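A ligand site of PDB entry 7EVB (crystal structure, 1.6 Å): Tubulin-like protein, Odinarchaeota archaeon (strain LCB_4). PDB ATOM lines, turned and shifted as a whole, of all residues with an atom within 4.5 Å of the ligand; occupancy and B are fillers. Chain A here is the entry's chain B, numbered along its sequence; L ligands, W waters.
Water W7 lies within hydrogen-bond range of OE1 of Gln 13 (2.7 Å) and O9 of the ligand (2.7 Å).
Water W5 lies within hydrogen-bond range of an oxygen (O5) of the ligand, the side-chain hydroxyl of Thr 138, the backbone NH of Gly 141 and the backbone NH of Gly 144.
Water W3 lies within hydrogen-bond range of O9 of the ligand and OD1 of Asn 102.
Water W10 lies within hydrogen-bond range of O13 of the ligand (3.1 Å), OD1 of Asp 176 (3.1 Å) and ND2 of Asn 203 (3.1 Å).
Water W1 lies within hydrogen-bond range of OD2 of Asp 69 (2.8 Å), O6 of the ligand (3.3 Å) and N of Gln 13 (3.5 Å).
Water W8 lies within hydrogen-bond range of O of Val 169 (2.9 Å) and O12 of the ligand (3.4 Å).
O8 of the ligand is in hydrogen-bond range of OG1 of Thr 138.
N of Asn 102 lies within hydrogen-bond range of O1 of the ligand (2.7 Å).
N of Gln 13 sits at hydrogen-bond distance from O6 of the ligand, 2.8 Å away.
The backbone NH (N) of Gly 142 lies within hydrogen-bond range of an oxygen (O1) of the ligand (3.0 Å).
OD1 of Asn 102 lies close to O1 of the ligand (2.8 Å).
NE2 of Gln 17 is in hydrogen-bond range of O14 of the ligand (2.9 Å).
The side-chain amide oxygen (OD1) of Asn 203 is in hydrogen-bond range of a nitrogen (N4) of the ligand (2.7 Å).
The backbone NH of Ala 100 is in hydrogen-bond range of an oxygen (O3) of the ligand (3.1 Å).
OG1 of Thr 143 is in hydrogen-bond range of O3 of the ligand, 2.7 Å away.
N of Gly 144 is in hydrogen-bond range of O5 of the ligand.
OD1 of Asn 226 sits at hydrogen-bond distance from N3 of the ligand.
OD2 of Asp 176 sits at hydrogen-bond distance from O13 of the ligand (2.6 Å).
The backbone NH of Gly 14 lies within hydrogen-bond range of an oxygen (O8) of the ligand.
N of Thr 143 is in hydrogen-bond range of O4 of the ligand (2.8 Å).
The side-chain amide nitrogen of Asn 226 lies close to the backbone carbonyl oxygen of Phe 222 (3.3 Å).
NE2 of Gln 13 is in hydrogen-bond range of OE1 of Gln 17, 2.9 Å away.
N of Gln 13 sits at hydrogen-bond distance from OD2 of Asp 69.
Merely in contact with the ligand: Phe 222, Gly 141, Gly 12 and His 101.
Hydrophobic or aromatic side chains that line the ligand: Ala 100 and Phe 222.
The nearest printed residue that does not touch the ligand is Val 177 (4.1 Å).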
ATOM      1  N   GLY A  12       4.562 -12.460  12.340  1.00  0.00           N
ATOM      2  CA  GLY A  12       5.024 -13.568  13.157  1.00  0.00           C
ATOM      3  C   GLY A  12       5.142 -13.193  14.624  1.00  0.00           C
ATOM      4  O   GLY A  12       4.847 -12.068  15.037  1.00  0.00           O
ATOM      5  N   GLN A  13       5.577 -14.165  15.443  1.00  0.00           N
ATOM      6  CA  GLN A  13       5.598 -13.945  16.887  1.00  0.00           C
ATOM      7  C   GLN A  13       6.524 -12.790  17.246  1.00  0.00           C
ATOM      8  O   GLN A  13       6.113 -11.838  17.937  1.00  0.00           O
ATOM      9  CB  GLN A  13       6.025 -15.207  17.636  1.00  0.00           C
ATOM     10  CG  GLN A  13       6.181 -14.952  19.163  1.00  0.00           C
ATOM     11  CD  GLN A  13       5.888 -16.170  20.016  1.00  0.00           C
ATOM     12  OE1 GLN A  13       6.043 -17.305  19.566  1.00  0.00           O
ATOM     13  NE2 GLN A  13       5.479 -15.947  21.266  1.00  0.00           N
ATOM     14  N   GLY A  14       7.768 -12.851  16.794  1.00  0.00           N
ATOM     15  CA  GLY A  14       8.718 -11.808  17.126  1.00  0.00           C
ATOM     16  C   GLY A  14       8.294 -10.444  16.598  1.00  0.00           C
ATOM     17  O   GLY A  14       8.362  -9.451  17.322  1.00  0.00           O
ATOM     18  N   GLN A  17       5.456  -9.111  18.781  1.00  0.00           N
ATOM     19  CA  GLN A  17       5.908  -8.761  20.130  1.00  0.00           C
ATOM     20  C   GLN A  17       6.768  -7.497  20.102  1.00  0.00           C
ATOM     21  O   GLN A  17       6.634  -6.647  20.997  1.00  0.00           O
ATOM     22  CB  GLN A  17       6.648  -9.948  20.755  1.00  0.00           C
ATOM     23  CG  GLN A  17       5.637 -11.081  21.002  1.00  0.00           C
ATOM     24  CD  GLN A  17       6.202 -12.366  21.588  1.00  0.00           C
ATOM     25  OE1 GLN A  17       5.430 -13.181  22.074  1.00  0.00           O
ATOM     26  NE2 GLN A  17       7.537 -12.565  21.550  1.00  0.00           N
ATOM     27  N   ILE A  18       7.590  -7.332  19.076  1.00  0.00           N
ATOM     28  CA  ILE A  18       8.349  -6.084  18.921  1.00  0.00           C
ATOM     29  C   ILE A  18       7.390  -4.919  18.730  1.00  0.00           C
ATOM     30  O   ILE A  18       7.616  -3.817  19.246  1.00  0.00           O
ATOM     31  CB  ILE A  18       9.342  -6.203  17.752  1.00  0.00           C
ATOM     32  CG1 ILE A  18      10.422  -7.225  18.082  1.00  0.00           C
ATOM     33  CG2 ILE A  18       9.970  -4.855  17.430  1.00  0.00           C
ATOM     34  CD1 ILE A  18      11.192  -7.684  16.853  1.00  0.00           C
ATOM     35  N   ASP A  69      -0.073 -12.807  11.462  1.00  0.00           N
ATOM     36  CA  ASP A  69       0.562 -14.059  11.867  1.00  0.00           C
ATOM     37  C   ASP A  69      -0.243 -15.219  11.317  1.00  0.00           C
ATOM     38  O   ASP A  69      -1.441 -15.094  11.031  1.00  0.00           O
ATOM     39  CB  ASP A  69       0.669 -14.159  13.393  1.00  0.00           C
ATOM     40  CG  ASP A  69       1.832 -15.026  13.868  1.00  0.00           C
ATOM     41  OD1 ASP A  69       2.339 -15.894  13.110  1.00  0.00           O
ATOM     42  OD2 ASP A  69       2.245 -14.846  15.028  1.00  0.00           O
ATOM     43  N   GLY A  99      -0.086 -22.096  11.424  1.00  0.00           N
ATOM     44  CA  GLY A  99       1.325 -21.929  11.714  1.00  0.00           C
ATOM     45  C   GLY A  99       2.226 -22.297  10.536  1.00  0.00           C
ATOM     46  O   GLY A  99       1.850 -23.031   9.631  1.00  0.00           O
ATOM     47  N   ALA A 100       3.443 -21.738  10.548  1.00  0.00           N
ATOM     48  CA  ALA A 100       4.410 -22.060   9.499  1.00  0.00           C
ATOM     49  C   ALA A 100       5.411 -23.134   9.905  1.00  0.00           C
ATOM     50  O   ALA A 100       6.194 -23.579   9.070  1.00  0.00           O
ATOM     51  CB  ALA A 100       5.192 -20.802   9.054  1.00  0.00           C
ATOM     52  N   HIS A 101       5.398 -23.556  11.175  1.00  0.00           N
ATOM     53  CA  HIS A 101       6.214 -24.679  11.654  1.00  0.00           C
ATOM     54  C   HIS A 101       7.697 -24.470  11.357  1.00  0.00           C
ATOM     55  O   HIS A 101       8.435 -25.421  11.065  1.00  0.00           O
ATOM     56  CB  HIS A 101       5.737 -26.008  11.074  1.00  0.00           C
ATOM     57  CG  HIS A 101       4.256 -26.169  11.084  1.00  0.00           C
ATOM     58  ND1 HIS A 101       3.493 -26.054  12.223  1.00  0.00           N
ATOM     59  CD2 HIS A 101       3.382 -26.443  10.075  1.00  0.00           C
ATOM     60  CE1 HIS A 101       2.218 -26.248  11.922  1.00  0.00           C
ATOM     61  NE2 HIS A 101       2.132 -26.488  10.631  1.00  0.00           N
ATOM     62  N   ASN A 102       8.124 -23.196  11.423  1.00  0.00           N
ATOM     63  CA  ASN A 102       9.529 -22.795  11.293  1.00  0.00           C
ATOM     64  C   ASN A 102      10.100 -23.070   9.908  1.00  0.00           C
ATOM     65  O   ASN A 102      11.314 -23.233   9.755  1.00  0.00           O
ATOM     66  CB  ASN A 102      10.404 -23.454  12.358  1.00  0.00           C
ATOM     67  CG  ASN A 102      10.343 -22.770  13.704  1.00  0.00           C
ATOM     68  OD1 ASN A 102       9.607 -21.766  13.928  1.00  0.00           O
ATOM     69  ND2 ASN A 102      11.095 -23.312  14.629  1.00  0.00           N
ATOM     70  N   THR A 138      11.148 -11.484  12.476  1.00  0.00           N
ATOM     71  CA  THR A 138      12.348 -12.296  12.680  1.00  0.00           C
ATOM     72  C   THR A 138      12.622 -13.112  11.427  1.00  0.00           C
ATOM     73  O   THR A 138      11.711 -13.414  10.639  1.00  0.00           O
ATOM     74  CB  THR A 138      12.203 -13.234  13.886  1.00  0.00           C
ATOM     75  OG1 THR A 138      11.230 -14.233  13.569  1.00  0.00           O
ATOM     76  CG2 THR A 138      11.763 -12.474  15.134  1.00  0.00           C
ATOM     77  N   GLY A 141      12.481 -17.926  12.238  1.00  0.00           N
ATOM     78  CA  GLY A 141      11.262 -18.700  12.231  1.00  0.00           C
ATOM     79  C   GLY A 141      10.713 -18.871  10.821  1.00  0.00           C
ATOM     80  O   GLY A 141      11.431 -18.712   9.829  1.00  0.00           O
ATOM     81  N   GLY A 142       9.427 -19.213  10.725  1.00  0.00           N
ATOM     82  CA  GLY A 142       8.817 -19.503   9.439  1.00  0.00           C
ATOM     83  C   GLY A 142       7.869 -18.440   8.903  1.00  0.00           C
ATOM     84  O   GLY A 142       7.763 -18.239   7.693  1.00  0.00           O
ATOM     85  N   THR A 143       7.163 -17.767   9.805  1.00  0.00           N
ATOM     86  CA  THR A 143       6.172 -16.788   9.377  1.00  0.00           C
ATOM     87  C   THR A 143       6.812 -15.418   9.137  1.00  0.00           C
ATOM     88  O   THR A 143       6.693 -14.853   8.039  1.00  0.00           O
ATOM     89  CB  THR A 143       5.054 -16.688  10.422  1.00  0.00           C
ATOM     90  OG1 THR A 143       4.373 -17.948  10.503  1.00  0.00           O
ATOM     91  CG2 THR A 143       4.055 -15.607  10.038  1.00  0.00           C
ATOM     92  N   GLY A 144       7.462 -14.867  10.159  1.00  0.00           N
ATOM     93  CA  GLY A 144       8.226 -13.644   9.960  1.00  0.00           C
ATOM     94  C   GLY A 144       9.158 -13.752   8.775  1.00  0.00           C
ATOM     95  O   GLY A 144       9.250 -12.824   7.968  1.00  0.00           O
ATOM     96  N   VAL A 169      15.253  -9.470  12.540  1.00  0.00           N
ATOM     97  CA  VAL A 169      16.033 -10.066  13.622  1.00  0.00           C
ATOM     98  C   VAL A 169      16.748 -11.309  13.107  1.00  0.00           C
ATOM     99  O   VAL A 169      16.096 -12.308  12.745  1.00  0.00           O
ATOM    100  CB  VAL A 169      15.150 -10.417  14.829  1.00  0.00           C
ATOM    101  CG1 VAL A 169      16.026 -10.871  15.994  1.00  0.00           C
ATOM    102  CG2 VAL A 169      14.331  -9.198  15.220  1.00  0.00           C
ATOM    103  N   ASP A 176      18.525 -20.645  18.017  1.00  0.00           N
ATOM    104  CA  ASP A 176      17.500 -21.323  18.797  1.00  0.00           C
ATOM    105  C   ASP A 176      16.377 -21.885  17.906  1.00  0.00           C
ATOM    106  O   ASP A 176      15.302 -22.242  18.402  1.00  0.00           O
ATOM    107  CB  ASP A 176      16.952 -20.405  19.879  1.00  0.00           C
ATOM    108  CG  ASP A 176      16.230 -19.208  19.336  1.00  0.00           C
ATOM    109  OD1 ASP A 176      16.594 -18.741  18.248  1.00  0.00           O
ATOM    110  OD2 ASP A 176      15.301 -18.743  20.016  1.00  0.00           O
ATOM    111  N   VAL A 177      16.629 -21.967  16.600  1.00  0.00           N
ATOM    112  CA  VAL A 177      15.844 -22.706  15.629  1.00  0.00           C
ATOM    113  C   VAL A 177      16.865 -23.393  14.732  1.00  0.00           C
ATOM    114  O   VAL A 177      17.678 -22.711  14.099  1.00  0.00           O
ATOM    115  CB  VAL A 177      14.934 -21.797  14.778  1.00  0.00           C
ATOM    116  CG1 VAL A 177      14.177 -22.602  13.723  1.00  0.00           C
ATOM    117  CG2 VAL A 177      13.979 -20.990  15.663  1.00  0.00           C
ATOM    118  N   ASN A 203      19.598 -11.331  18.871  1.00  0.00           N
ATOM    119  CA  ASN A 203      19.355 -11.404  20.304  1.00  0.00           C
ATOM    120  C   ASN A 203      20.628 -11.543  21.116  1.00  0.00           C
ATOM    121  O   ASN A 203      20.631 -11.168  22.289  1.00  0.00           O
ATOM    122  CB  ASN A 203      18.400 -12.546  20.603  1.00  0.00           C
ATOM    123  CG  ASN A 203      17.017 -12.242  20.119  1.00  0.00           C
ATOM    124  OD1 ASN A 203      16.705 -11.081  19.856  1.00  0.00           O
ATOM    125  ND2 ASN A 203      16.184 -13.266  19.973  1.00  0.00           N
ATOM    126  N   LEU A 206      21.481  -7.957  21.587  1.00  0.00           N
ATOM    127  CA  LEU A 206      20.490  -7.290  22.413  1.00  0.00           C
ATOM    128  C   LEU A 206      20.608  -7.695  23.874  1.00  0.00           C
ATOM    129  O   LEU A 206      20.546  -6.850  24.776  1.00  0.00           O
ATOM    130  CB  LEU A 206      19.087  -7.568  21.885  1.00  0.00           C
ATOM    131  CG  LEU A 206      18.751  -7.031  20.495  1.00  0.00           C
ATOM    132  CD1 LEU A 206      17.337  -7.433  20.076  1.00  0.00           C
ATOM    133  CD2 LEU A 206      18.922  -5.499  20.421  1.00  0.00           C
ATOM    134  N   PHE A 222      10.191 -10.941  26.530  1.00  0.00           N
ATOM    135  CA  PHE A 222      10.851 -10.280  25.408  1.00  0.00           C
ATOM    136  C   PHE A 222      10.651  -8.770  25.412  1.00  0.00           C
ATOM    137  O   PHE A 222      11.375  -8.070  24.697  1.00  0.00           O
ATOM    138  CB  PHE A 222      10.374 -10.848  24.066  1.00  0.00           C
ATOM    139  CG  PHE A 222      11.252 -11.938  23.517  1.00  0.00           C
ATOM    140  CD1 PHE A 222      12.611 -11.736  23.334  1.00  0.00           C
ATOM    141  CD2 PHE A 222      10.709 -13.168  23.161  1.00  0.00           C
ATOM    142  CE1 PHE A 222      13.428 -12.734  22.824  1.00  0.00           C
ATOM    143  CE2 PHE A 222      11.523 -14.174  22.653  1.00  0.00           C
ATOM    144  CZ  PHE A 222      12.885 -13.956  22.489  1.00  0.00           C
ATOM    145  N   ASN A 226      12.945  -6.223  23.443  1.00  0.00           N
ATOM    146  CA  ASN A 226      12.453  -5.579  22.232  1.00  0.00           C
ATOM    147  C   ASN A 226      12.407  -4.064  22.336  1.00  0.00           C
ATOM    148  O   ASN A 226      12.306  -3.395  21.312  1.00  0.00           O
ATOM    149  CB  ASN A 226      11.044  -6.081  21.910  1.00  0.00           C
ATOM    150  CG  ASN A 226      11.027  -7.534  21.541  1.00  0.00           C
ATOM    151  OD1 ASN A 226      12.031  -8.074  21.087  1.00  0.00           O
ATOM    152  ND2 ASN A 226       9.877  -8.170  21.714  1.00  0.00           N
ATOM    153  N   ILE A 229      14.829  -2.406  20.023  1.00  0.00           N
ATOM    154  CA  ILE A 229      14.427  -2.310  18.622  1.00  0.00           C
ATOM    155  C   ILE A 229      13.440  -1.167  18.439  1.00  0.00           C
ATOM    156  O   ILE A 229      13.534  -0.384  17.485  1.00  0.00           O
ATOM    157  CB  ILE A 229      13.839  -3.645  18.137  1.00  0.00           C
ATOM    158  CG1 ILE A 229      14.863  -4.771  18.333  1.00  0.00           C
ATOM    159  CG2 ILE A 229      13.403  -3.569  16.678  1.00  0.00           C
ATOM    160  CD1 ILE A 229      14.331  -6.148  17.929  1.00  0.00           C
HETATM  161  P1  LIG L   1       6.563 -19.708  12.948  1.00  0.00           P
HETATM  162  O1  LIG L   1       7.486 -20.752  12.377  1.00  0.00           O
HETATM  163  O2  LIG L   1       6.436 -19.841  14.456  1.00  0.00           O
HETATM  164  O3  LIG L   1       5.224 -19.784  12.256  1.00  0.00           O
HETATM  165  O4  LIG L   1       7.231 -18.282  12.567  1.00  0.00           O
HETATM  166  P2  LIG L   1       7.378 -16.985  13.528  1.00  0.00           P
HETATM  167  O5  LIG L   1       7.731 -15.829  12.630  1.00  0.00           O
HETATM  168  O6  LIG L   1       6.160 -16.738  14.381  1.00  0.00           O
HETATM  169  O7  LIG L   1       8.644 -17.386  14.426  1.00  0.00           O
HETATM  170  P3  LIG L   1       9.356 -16.508  15.573  1.00  0.00           P
HETATM  171  O8  LIG L   1       9.062 -15.046  15.417  1.00  0.00           O
HETATM  172  O9  LIG L   1       9.036 -17.116  16.927  1.00  0.00           O
HETATM  173  O10 LIG L   1      10.887 -16.803  15.158  1.00  0.00           O
HETATM  174  C1  LIG L   1      11.790 -17.478  15.992  1.00  0.00           C
HETATM  175  C2  LIG L   1      13.020 -16.599  16.134  1.00  0.00           C
HETATM  176  O11 LIG L   1      12.616 -15.317  16.577  1.00  0.00           O
HETATM  177  C3  LIG L   1      13.940 -17.173  17.194  1.00  0.00           C
HETATM  178  O12 LIG L   1      15.253 -16.887  16.767  1.00  0.00           O
HETATM  179  C4  LIG L   1      13.495 -16.415  18.434  1.00  0.00           C
HETATM  180  O13 LIG L   1      14.488 -16.301  19.408  1.00  0.00           O
HETATM  181  C5  LIG L   1      13.131 -15.058  17.863  1.00  0.00           C
HETATM  182  N1  LIG L   1      12.050 -14.328  18.542  1.00  0.00           N
HETATM  183  C6  LIG L   1      10.740 -14.727  18.723  1.00  0.00           C
HETATM  184  N2  LIG L   1      10.087 -13.705  19.337  1.00  0.00           N
HETATM  185  C7  LIG L   1      10.954 -12.685  19.534  1.00  0.00           C
HETATM  186  C8  LIG L   1      10.808 -11.420  20.094  1.00  0.00           C
HETATM  187  O14 LIG L   1       9.734 -11.032  20.555  1.00  0.00           O
HETATM  188  N3  LIG L   1      11.902 -10.584  20.133  1.00  0.00           N
HETATM  189  C9  LIG L   1      13.125 -10.990  19.629  1.00  0.00           C
HETATM  190  N4  LIG L   1      14.176 -10.160  19.681  1.00  0.00           N
HETATM  191  N5  LIG L   1      13.264 -12.242  19.070  1.00  0.00           N
HETATM  192  C10 LIG L   1      12.183 -13.064  19.021  1.00  0.00           C
HETATM  193  O   HOH W   1       3.575 -16.852  16.394  1.00  0.00           O
HETATM  194  O   HOH W   2      16.003 -14.427  16.475  1.00  0.00           O
HETATM  195  O   HOH W   3       9.420 -19.988  16.833  1.00  0.00           O
HETATM  196  O   HOH W   4      16.602 -17.451  14.727  1.00  0.00           O
HETATM  197  O   HOH W   5      10.292 -15.856  11.369  1.00  0.00           O
HETATM  198  O   HOH W   6       8.585 -12.738  13.478  1.00  0.00           O
HETATM  199  O   HOH W   7       6.664 -18.387  17.219  1.00  0.00           O
HETATM  200  O   HOH W   8      15.720 -14.896  14.078  1.00  0.00           O
HETATM  201  O   HOH W   9       3.647 -18.170  13.651  1.00  0.00           O
HETATM  202  O   HOH W  10      17.486 -15.871  18.944  1.00  0.00           O
